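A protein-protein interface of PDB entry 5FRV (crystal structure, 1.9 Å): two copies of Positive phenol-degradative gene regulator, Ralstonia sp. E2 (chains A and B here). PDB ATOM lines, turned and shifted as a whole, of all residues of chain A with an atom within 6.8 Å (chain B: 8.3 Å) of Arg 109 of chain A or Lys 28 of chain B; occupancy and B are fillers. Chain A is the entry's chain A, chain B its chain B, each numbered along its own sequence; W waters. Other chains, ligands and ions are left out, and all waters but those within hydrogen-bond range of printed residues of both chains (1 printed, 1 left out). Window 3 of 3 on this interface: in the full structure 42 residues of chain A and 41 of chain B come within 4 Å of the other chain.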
ATOM      1  N   SER A   9      -5.998 -23.774 -18.003  1.00  0.00           N
ATOM      2  CA  SER A   9      -6.257 -22.924 -19.160  1.00  0.00           C
ATOM      3  C   SER A   9      -5.031 -22.820 -20.063  1.00  0.00           C
ATOM      4  O   SER A   9      -4.034 -22.205 -19.688  1.00  0.00           O
ATOM      5  CB  SER A   9      -6.686 -21.517 -18.716  1.00  0.00           C
ATOM      6  OG  SER A   9      -5.658 -20.841 -18.011  1.00  0.00           O
ATOM      7  N   MET A  12      -7.643 -21.865 -23.716  1.00  0.00           N
ATOM      8  CA  MET A  12      -8.650 -20.948 -23.170  1.00  0.00           C
ATOM      9  C   MET A  12      -8.151 -19.507 -22.973  1.00  0.00           C
ATOM     10  O   MET A  12      -8.899 -18.559 -23.226  1.00  0.00           O
ATOM     11  CB  MET A  12      -9.182 -21.478 -21.833  1.00  0.00           C
ATOM     12  CG  MET A  12      -9.909 -22.818 -21.916  1.00  0.00           C
ATOM     13  SD  MET A  12     -11.581 -22.735 -22.608  1.00  0.00           S
ATOM     14  CE  MET A  12     -12.497 -21.980 -21.277  1.00  0.00           C
ATOM     15  N   LEU A  16      -9.850 -16.376 -24.737  1.00  0.00           N
ATOM     16  CA  LEU A  16     -10.264 -15.286 -23.854  1.00  0.00           C
ATOM     17  C   LEU A  16      -9.609 -13.968 -24.246  1.00  0.00           C
ATOM     18  O   LEU A  16     -10.233 -12.910 -24.182  1.00  0.00           O
ATOM     19  CB  LEU A  16      -9.933 -15.618 -22.395  1.00  0.00           C
ATOM     20  CG  LEU A  16     -10.824 -16.652 -21.689  1.00  0.00           C
ATOM     21  CD1 LEU A  16     -10.196 -17.137 -20.381  1.00  0.00           C
ATOM     22  CD2 LEU A  16     -12.200 -16.082 -21.414  1.00  0.00           C
ATOM     23  N   PRO A  99     -17.227 -21.974 -24.721  1.00  0.00           N
ATOM     24  CA  PRO A  99     -16.877 -21.930 -23.295  1.00  0.00           C
ATOM     25  C   PRO A  99     -16.188 -20.612 -22.917  1.00  0.00           C
ATOM     26  O   PRO A  99     -16.428 -20.076 -21.832  1.00  0.00           O
ATOM     27  CB  PRO A  99     -15.935 -23.130 -23.129  1.00  0.00           C
ATOM     28  CG  PRO A  99     -16.405 -24.111 -24.148  1.00  0.00           C
ATOM     29  CD  PRO A  99     -16.860 -23.264 -25.341  1.00  0.00           C
ATOM     30  N   HIS A 102     -19.066 -17.803 -22.820  1.00  0.00           N
ATOM     31  CA  HIS A 102     -19.806 -18.028 -21.625  1.00  0.00           C
ATOM     32  C   HIS A 102     -19.149 -17.491 -20.367  1.00  0.00           C
ATOM     33  O   HIS A 102     -19.794 -16.995 -19.505  1.00  0.00           O
ATOM     34  CB  HIS A 102     -20.123 -19.489 -21.431  1.00  0.00           C
ATOM     35  CG  HIS A 102     -21.571 -19.745 -21.245  1.00  0.00           C
ATOM     36  ND1 HIS A 102     -22.099 -20.993 -21.161  1.00  0.00           N
ATOM     37  CD2 HIS A 102     -22.606 -18.892 -21.167  1.00  0.00           C
ATOM     38  CE1 HIS A 102     -23.399 -20.908 -21.044  1.00  0.00           C
ATOM     39  NE2 HIS A 102     -23.735 -19.643 -21.043  1.00  0.00           N
ATOM     40  N   THR A 103     -17.853 -17.632 -20.312  1.00  0.00           N
ATOM     41  CA  THR A 103     -17.039 -17.138 -19.194  1.00  0.00           C
ATOM     42  C   THR A 103     -16.864 -15.619 -19.197  1.00  0.00           C
ATOM     43  O   THR A 103     -17.023 -14.979 -18.152  1.00  0.00           O
ATOM     44  CB  THR A 103     -15.633 -17.811 -19.194  1.00  0.00           C
ATOM     45  OG1 THR A 103     -15.783 -19.232 -19.198  1.00  0.00           O
ATOM     46  CG2 THR A 103     -14.833 -17.413 -17.973  1.00  0.00           C
ATOM     47  N   GLY A 106     -19.690 -13.817 -17.920  1.00  0.00           N
ATOM     48  CA  GLY A 106     -19.860 -13.920 -16.474  1.00  0.00           C
ATOM     49  C   GLY A 106     -20.960 -14.879 -16.052  1.00  0.00           C
ATOM     50  O   GLY A 106     -21.514 -14.780 -14.956  1.00  0.00           O
ATOM     51  N   VAL A 107     -21.294 -15.801 -16.944  1.00  0.00           N
ATOM     52  CA  VAL A 107     -22.390 -16.727 -16.706  1.00  0.00           C
ATOM     53  C   VAL A 107     -21.898 -17.906 -15.843  1.00  0.00           C
ATOM     54  O   VAL A 107     -22.579 -18.348 -14.907  1.00  0.00           O
ATOM     55  CB  VAL A 107     -22.985 -17.173 -18.069  1.00  0.00           C
ATOM     56  CG1 VAL A 107     -23.932 -18.356 -17.936  1.00  0.00           C
ATOM     57  CG2 VAL A 107     -23.704 -15.972 -18.744  1.00  0.00           C
ATOM     58  N   VAL A 108     -20.689 -18.371 -16.136  1.00  0.00           N
ATOM     59  CA  VAL A 108     -20.136 -19.584 -15.540  1.00  0.00           C
ATOM     60  C   VAL A 108     -18.675 -19.697 -15.972  1.00  0.00           C
ATOM     61  O   VAL A 108     -18.278 -19.139 -17.000  1.00  0.00           O
ATOM     62  CB  VAL A 108     -20.941 -20.872 -15.947  1.00  0.00           C
ATOM     63  CG1 VAL A 108     -20.961 -21.080 -17.465  1.00  0.00           C
ATOM     64  CG2 VAL A 108     -20.391 -22.140 -15.261  1.00  0.00           C
ATOM     65  N   ARG A 109     -17.866 -20.379 -15.168  1.00  0.00           N
ATOM     66  CA  ARG A 109     -16.512 -20.732 -15.574  1.00  0.00           C
ATOM     67  C   ARG A 109     -16.558 -22.116 -16.190  1.00  0.00           C
ATOM     68  O   ARG A 109     -16.989 -23.084 -15.555  1.00  0.00           O
ATOM     69  CB  ARG A 109     -15.539 -20.705 -14.394  1.00  0.00           C
ATOM     70  CG  ARG A 109     -14.156 -21.213 -14.769  1.00  0.00           C
ATOM     71  CD  ARG A 109     -13.258 -21.439 -13.556  1.00  0.00           C
ATOM     72  NE  ARG A 109     -11.988 -22.031 -13.977  1.00  0.00           N
ATOM     73  CZ  ARG A 109     -10.954 -21.332 -14.435  1.00  0.00           C
ATOM     74  NH1 ARG A 109     -11.029 -20.008 -14.512  1.00  0.00           N
ATOM     75  NH2 ARG A 109      -9.839 -21.951 -14.809  1.00  0.00           N
ATOM     76  N   VAL A 110     -16.128 -22.210 -17.438  1.00  0.00           N
ATOM     77  CA  VAL A 110     -16.279 -23.450 -18.185  1.00  0.00           C
ATOM     78  C   VAL A 110     -14.931 -24.101 -18.380  1.00  0.00           C
ATOM     79  O   VAL A 110     -13.960 -23.439 -18.755  1.00  0.00           O
ATOM     80  CB  VAL A 110     -16.932 -23.205 -19.540  1.00  0.00           C
ATOM     81  CG1 VAL A 110     -17.297 -24.540 -20.218  1.00  0.00           C
ATOM     82  CG2 VAL A 110     -18.160 -22.327 -19.361  1.00  0.00           C
ATOM     83  N   THR A 111     -14.867 -25.395 -18.094  1.00  0.00           N
ATOM     84  CA  THR A 111     -13.685 -26.184 -18.426  1.00  0.00           C
ATOM     85  C   THR A 111     -14.063 -27.391 -19.274  1.00  0.00           C
ATOM     86  O   THR A 111     -14.774 -28.288 -18.803  1.00  0.00           O
ATOM     87  CB  THR A 111     -12.953 -26.659 -17.163  1.00  0.00           C
ATOM     88  OG1 THR A 111     -12.692 -25.529 -16.324  1.00  0.00           O
ATOM     89  CG2 THR A 111     -11.634 -27.340 -17.531  1.00  0.00           C
ATOM     90  N   LEU A 129     -17.008 -29.140 -17.553  1.00  0.00           N
ATOM     91  CA  LEU A 129     -17.146 -28.717 -16.162  1.00  0.00           C
ATOM     92  C   LEU A 129     -17.626 -27.265 -16.081  1.00  0.00           C
ATOM     93  O   LEU A 129     -17.145 -26.394 -16.822  1.00  0.00           O
ATOM     94  CB  LEU A 129     -15.818 -28.854 -15.422  1.00  0.00           C
ATOM     95  CG  LEU A 129     -15.823 -28.407 -13.954  1.00  0.00           C
ATOM     96  CD1 LEU A 129     -16.641 -29.377 -13.096  1.00  0.00           C
ATOM     97  CD2 LEU A 129     -14.410 -28.258 -13.398  1.00  0.00           C
ATOM     98  N   TRP A 130     -18.567 -27.026 -15.176  1.00  0.00           N
ATOM     99  CA  TRP A 130     -19.104 -25.697 -14.890  1.00  0.00           C
ATOM    100  C   TRP A 130     -18.832 -25.283 -13.444  1.00  0.00           C
ATOM    101  O   TRP A 130     -19.450 -25.812 -12.520  1.00  0.00           O
ATOM    102  CB  TRP A 130     -20.610 -25.673 -15.138  1.00  0.00           C
ATOM    103  CG  TRP A 130     -21.037 -25.416 -16.559  1.00  0.00           C
ATOM    104  CD1 TRP A 130     -20.248 -25.032 -17.601  1.00  0.00           C
ATOM    105  CD2 TRP A 130     -22.371 -25.521 -17.080  1.00  0.00           C
ATOM    106  NE1 TRP A 130     -21.011 -24.888 -18.744  1.00  0.00           N
ATOM    107  CE2 TRP A 130     -22.317 -25.182 -18.442  1.00  0.00           C
ATOM    108  CE3 TRP A 130     -23.609 -25.848 -16.519  1.00  0.00           C
ATOM    109  CZ2 TRP A 130     -23.449 -25.168 -19.248  1.00  0.00           C
ATOM    110  CZ3 TRP A 130     -24.731 -25.861 -17.334  1.00  0.00           C
ATOM    111  CH2 TRP A 130     -24.643 -25.510 -18.677  1.00  0.00           C
ATOM    112  N   GLU A 131     -17.933 -24.328 -13.239  1.00  0.00           N
ATOM    113  CA  GLU A 131     -17.736 -23.793 -11.889  1.00  0.00           C
ATOM    114  C   GLU A 131     -18.315 -22.387 -11.749  1.00  0.00           C
ATOM    115  O   GLU A 131     -18.216 -21.574 -12.668  1.00  0.00           O
ATOM    116  CB  GLU A 131     -16.251 -23.804 -11.539  1.00  0.00           C
ATOM    117  CG  GLU A 131     -15.656 -25.216 -11.508  1.00  0.00           C
ATOM    118  CD  GLU A 131     -14.146 -25.216 -11.323  1.00  0.00           C
ATOM    119  OE1 GLU A 131     -13.424 -25.112 -12.343  1.00  0.00           O
ATOM    120  OE2 GLU A 131     -13.680 -25.308 -10.160  1.00  0.00           O
ATOM    121  N   ASP A 132     -18.936 -22.127 -10.600  1.00  0.00           N
ATOM    122  CA  ASP A 132     -19.536 -20.824 -10.274  1.00  0.00           C
ATOM    123  C   ASP A 132     -20.688 -20.439 -11.214  1.00  0.00           C
ATOM    124  O   ASP A 132     -20.832 -19.264 -11.577  1.00  0.00           O
ATOM    125  CB  ASP A 132     -18.473 -19.719 -10.295  1.00  0.00           C
ATOM    126  CG  ASP A 132     -17.214 -20.109  -9.543  1.00  0.00           C
ATOM    127  OD1 ASP A 132     -17.267 -20.204  -8.295  1.00  0.00           O
ATOM    128  OD2 ASP A 132     -16.171 -20.335 -10.203  1.00  0.00           O
ATOM    129  N   SER A 133     -21.506 -21.421 -11.590  1.00  0.00           N
ATOM    130  CA  SER A 133     -22.703 -21.156 -12.380  1.00  0.00           C
ATOM    131  C   SER A 133     -23.544 -20.084 -11.691  1.00  0.00           C
ATOM    132  O   SER A 133     -23.984 -20.283 -10.555  1.00  0.00           O
ATOM    133  CB  SER A 133     -23.528 -22.426 -12.562  1.00  0.00           C
ATOM    134  OG  SER A 133     -22.764 -23.459 -13.185  1.00  0.00           O
ATOM    135  N   PHE A 134     -23.771 -18.952 -12.357  1.00  0.00           N
ATOM    136  CA  PHE A 134     -24.623 -17.943 -11.753  1.00  0.00           C
ATOM    137  C   PHE A 134     -26.015 -18.508 -11.554  1.00  0.00           C
ATOM    138  O   PHE A 134     -26.688 -18.212 -10.575  1.00  0.00           O
ATOM    139  CB  PHE A 134     -24.691 -16.670 -12.610  1.00  0.00           C
ATOM    140  CG  PHE A 134     -25.859 -16.634 -13.565  1.00  0.00           C
ATOM    141  CD1 PHE A 134     -25.749 -17.176 -14.832  1.00  0.00           C
ATOM    142  CD2 PHE A 134     -27.068 -16.053 -13.191  1.00  0.00           C
ATOM    143  CE1 PHE A 134     -26.816 -17.146 -15.706  1.00  0.00           C
ATOM    144  CE2 PHE A 134     -28.139 -16.031 -14.046  1.00  0.00           C
ATOM    145  CZ  PHE A 134     -28.016 -16.573 -15.312  1.00  0.00           C
ATOM    146  N   ARG B  24     -16.023  -4.917 -12.431  1.00  0.00           N
ATOM    147  CA  ARG B  24     -14.902  -5.838 -12.274  1.00  0.00           C
ATOM    148  C   ARG B  24     -15.111  -7.200 -12.964  1.00  0.00           C
ATOM    149  O   ARG B  24     -16.128  -7.866 -12.752  1.00  0.00           O
ATOM    150  CB  ARG B  24     -14.670  -6.023 -10.772  1.00  0.00           C
ATOM    151  CG  ARG B  24     -13.399  -6.689 -10.367  1.00  0.00           C
ATOM    152  CD  ARG B  24     -13.106  -6.324  -8.919  1.00  0.00           C
ATOM    153  NE  ARG B  24     -14.275  -6.497  -8.055  1.00  0.00           N
ATOM    154  CZ  ARG B  24     -14.608  -7.648  -7.479  1.00  0.00           C
ATOM    155  NH1 ARG B  24     -13.863  -8.728  -7.676  1.00  0.00           N
ATOM    156  NH2 ARG B  24     -15.684  -7.727  -6.708  1.00  0.00           N
ATOM    157  N   PHE B  25     -14.145  -7.619 -13.779  1.00  0.00           N
ATOM    158  CA  PHE B  25     -14.249  -8.898 -14.482  1.00  0.00           C
ATOM    159  C   PHE B  25     -13.366  -9.974 -13.855  1.00  0.00           C
ATOM    160  O   PHE B  25     -12.158 -10.002 -14.082  1.00  0.00           O
ATOM    161  CB  PHE B  25     -13.889  -8.722 -15.961  1.00  0.00           C
ATOM    162  CG  PHE B  25     -15.022  -8.200 -16.808  1.00  0.00           C
ATOM    163  CD1 PHE B  25     -15.584  -6.960 -16.556  1.00  0.00           C
ATOM    164  CD2 PHE B  25     -15.516  -8.948 -17.867  1.00  0.00           C
ATOM    165  CE1 PHE B  25     -16.631  -6.476 -17.334  1.00  0.00           C
ATOM    166  CE2 PHE B  25     -16.558  -8.468 -18.651  1.00  0.00           C
ATOM    167  CZ  PHE B  25     -17.112  -7.222 -18.387  1.00  0.00           C
ATOM    168  N   ALA B  26     -13.986 -10.867 -13.087  1.00  0.00           N
ATOM    169  CA  ALA B  26     -13.294 -11.975 -12.424  1.00  0.00           C
ATOM    170  C   ALA B  26     -13.324 -13.270 -13.254  1.00  0.00           C
ATOM    171  O   ALA B  26     -14.039 -14.224 -12.923  1.00  0.00           O
ATOM    172  CB  ALA B  26     -13.909 -12.207 -11.052  1.00  0.00           C
ATOM    173  N   MET B  27     -12.527 -13.309 -14.316  1.00  0.00           N
ATOM    174  CA  MET B  27     -12.594 -14.388 -15.288  1.00  0.00           C
ATOM    175  C   MET B  27     -12.178 -15.727 -14.689  1.00  0.00           C
ATOM    176  O   MET B  27     -12.588 -16.779 -15.173  1.00  0.00           O
ATOM    177  CB  MET B  27     -11.715 -14.076 -16.505  1.00  0.00           C
ATOM    178  CG  MET B  27     -12.446 -13.390 -17.659  1.00  0.00           C
ATOM    179  SD  MET B  27     -11.403 -13.221 -19.130  1.00  0.00           S
ATOM    180  CE  MET B  27     -11.642 -11.489 -19.541  1.00  0.00           C
ATOM    181  N   LYS B  28     -11.366 -15.685 -13.636  1.00  0.00           N
ATOM    182  CA  LYS B  28     -10.937 -16.915 -12.978  1.00  0.00           C
ATOM    183  C   LYS B  28     -12.130 -17.606 -12.323  1.00  0.00           C
ATOM    184  O   LYS B  28     -12.160 -18.831 -12.205  1.00  0.00           O
ATOM    185  CB  LYS B  28      -9.841 -16.634 -11.943  1.00  0.00           C
ATOM    186  CG  LYS B  28      -9.846 -15.204 -11.387  1.00  0.00           C
ATOM    187  CD  LYS B  28      -8.502 -14.848 -10.746  1.00  0.00           C
ATOM    188  CE  LYS B  28      -8.471 -13.402 -10.259  1.00  0.00           C
ATOM    189  NZ  LYS B  28      -7.072 -12.881 -10.180  1.00  0.00           N
ATOM    190  N   GLU B  29     -13.114 -16.823 -11.899  1.00  0.00           N
ATOM    191  CA  GLU B  29     -14.293 -17.396 -11.267  1.00  0.00           C
ATOM    192  C   GLU B  29     -15.532 -17.244 -12.159  1.00  0.00           C
ATOM    193  O   GLU B  29     -16.664 -17.382 -11.688  1.00  0.00           O
ATOM    194  CB  GLU B  29     -14.514 -16.762  -9.892  1.00  0.00           C
ATOM    195  CG  GLU B  29     -15.015 -17.765  -8.859  1.00  0.00           C
ATOM    196  CD  GLU B  29     -14.250 -17.717  -7.552  1.00  0.00           C
ATOM    197  OE1 GLU B  29     -14.276 -16.658  -6.884  1.00  0.00           O
ATOM    198  OE2 GLU B  29     -13.619 -18.741  -7.195  1.00  0.00           O
ATOM    199  N   GLY B  30     -15.295 -16.997 -13.450  1.00  0.00           N
ATOM    200  CA  GLY B  30     -16.349 -16.805 -14.442  1.00  0.00           C
ATOM    201  C   GLY B  30     -17.395 -15.764 -14.058  1.00  0.00           C
ATOM    202  O   GLY B  30     -18.583 -15.925 -14.342  1.00  0.00           O
ATOM    203  N   SER B  31     -16.956 -14.690 -13.418  1.00  0.00           N
ATOM    204  CA  SER B  31     -17.884 -13.751 -12.801  1.00  0.00           C
ATOM    205  C   SER B  31     -17.597 -12.303 -13.137  1.00  0.00           C
ATOM    206  O   SER B  31     -16.458 -11.926 -13.401  1.00  0.00           O
ATOM    207  CB  SER B  31     -17.873 -13.931 -11.280  1.00  0.00           C
ATOM    208  OG  SER B  31     -18.368 -15.209 -10.952  1.00  0.00           O
ATOM    209  N   ARG B  38     -23.346  -9.473  -8.388  1.00  0.00           N
ATOM    210  CA  ARG B  38     -22.942 -10.254  -9.538  1.00  0.00           C
ATOM    211  C   ARG B  38     -23.789  -9.852 -10.745  1.00  0.00           C
ATOM    212  O   ARG B  38     -25.003  -9.675 -10.627  1.00  0.00           O
ATOM    213  CB  ARG B  38     -23.073 -11.742  -9.248  1.00  0.00           C
ATOM    214  CG  ARG B  38     -22.471 -12.577 -10.333  1.00  0.00           C
ATOM    215  CD  ARG B  38     -22.328 -14.033  -9.956  1.00  0.00           C
ATOM    216  NE  ARG B  38     -21.885 -14.742 -11.143  1.00  0.00           N
ATOM    217  CZ  ARG B  38     -21.640 -16.043 -11.206  1.00  0.00           C
ATOM    218  NH1 ARG B  38     -21.781 -16.820 -10.124  1.00  0.00           N
ATOM    219  NH2 ARG B  38     -21.261 -16.559 -12.365  1.00  0.00           N
HETATM  220  O   HOH W   1     -21.236 -12.884 -13.360  1.00  0.00           O
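The guanidinium group (NH2) of Arg 38 of chain B sits at hydrogen-bond distance from the backbone carbonyl oxygen (O) of Gly 106 of chain A, 3.2 Å away.
O of Val 107 of chain A is in hydrogen-bond range of NH2 of Arg 38 of chain B (3.4 Å).
NH1 of Arg 109 of chain A is in hydrogen-bond range of O of Lys 28 of chain B.
The backbone carbonyl oxygen of Asp 132 of chain A sits at hydrogen-bond distance from the guanidinium group of Arg 38 of chain B (2.8 Å).
The backbone carbonyl oxygen (O) of Gly 106 of chain A lies close to the backbone carbonyl oxygen (O) of Gly 30 of chain B.
O of Glu 29 of chain B sits close to OD2 of Asp 132 of chain A, 3.3 Å away.
N of Phe 134 of chain A lies close to NH2 of Arg 38 of chain B (3.5 Å).
Among the printed residues, merely in contact across the chains: Thr 103 of chain A with Met 27 of chain B, Arg 109 of chain A with Met 27 of chain B, Val 108 of chain A with Gly 30 of chain B, Leu 16 of chain A with Met 27 of chain B, Val 107 of chain A with Gly 30 of chain B, Arg 109 of chain A with Gly 30 of chain B and Thr 103 of chain A with Gly 30 of chain B.
Printed residues of chain A that touch a printed residue of chain B: Leu 16, Thr 103, Gly 106, Val 107, Val 108, Arg 109, Asp 132 and Phe 134.
Hydrophobic or aromatic side chains of chain B within 4 Å of the printed part of chain A: Met 27.
Among the printed residues, no Asp or Glu carboxylate lies within 4 Å of a Lys or Arg side-chain nitrogen of the other chain.
Water W1 bridges O of Gly 106 of chain A (2.5 Å) and NE of Arg 38 of chain B (3.0 Å).
The backbone NH of Val 107 of chain A is in hydrogen-bond range of the backbone carbonyl oxygen of His 102 of chain A, at 3.2 Å.
OG1 of Thr 103 of chain A sits close to O of Val 108 of chain A, 3.3 Å away.
OG1 of Thr 103 of chain A is in hydrogen-bond range of N of Val 110 of chain A (3.5 Å).
O of Val 107 of chain A lies within hydrogen-bond range of N of Phe 134 of chain A (2.9 Å).
NE of Arg 109 of chain A lies within salt-bridge range of OE1 of Glu 131 of chain A (3.8 Å).
O of Gly 30 of chain B lies within hydrogen-bond range of NH2 of Arg 38 of chain B.
No position is printed for both chains.
Of the 14 pairs that touch across the chains among the printed residues, none has its exchanged pair printed and touching as well.
Of chain B, only Met 27, Lys 28 and Gly 30 come within 4 Å of Arg 109 of chain A.
Of chain A, only Arg 109 (2.8 Å) comes within 4 Å of Lys 28 of chain B.
Val 108 of chain A touches one residue of chain B.
Printed residues of chain A within 4 Å of Arg 38 of chain B: Gly 106 (3.2 Å), Val 107 (3.4 Å), Asp 132 (2.8 Å) and Phe 134 (3.4 Å).
Printed residues of chain B within 4 Å of Phe 134 of chain A: Arg 38 (3.4 Å).
Printed residues of chain B within 4 Å of Leu 16 of chain A: Met 27.
Of the printed residues of chain B, Gly 106 of chain A touches Gly 30 (3.1 Å) and Arg 38 (3.2 Å).
Phe 25 of chain B touches none of the printed residues of chain A.
The nearest printed residue of chain A that does not touch Glu 29 of chain B is Arg 109 of chain A (4.1 Å).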
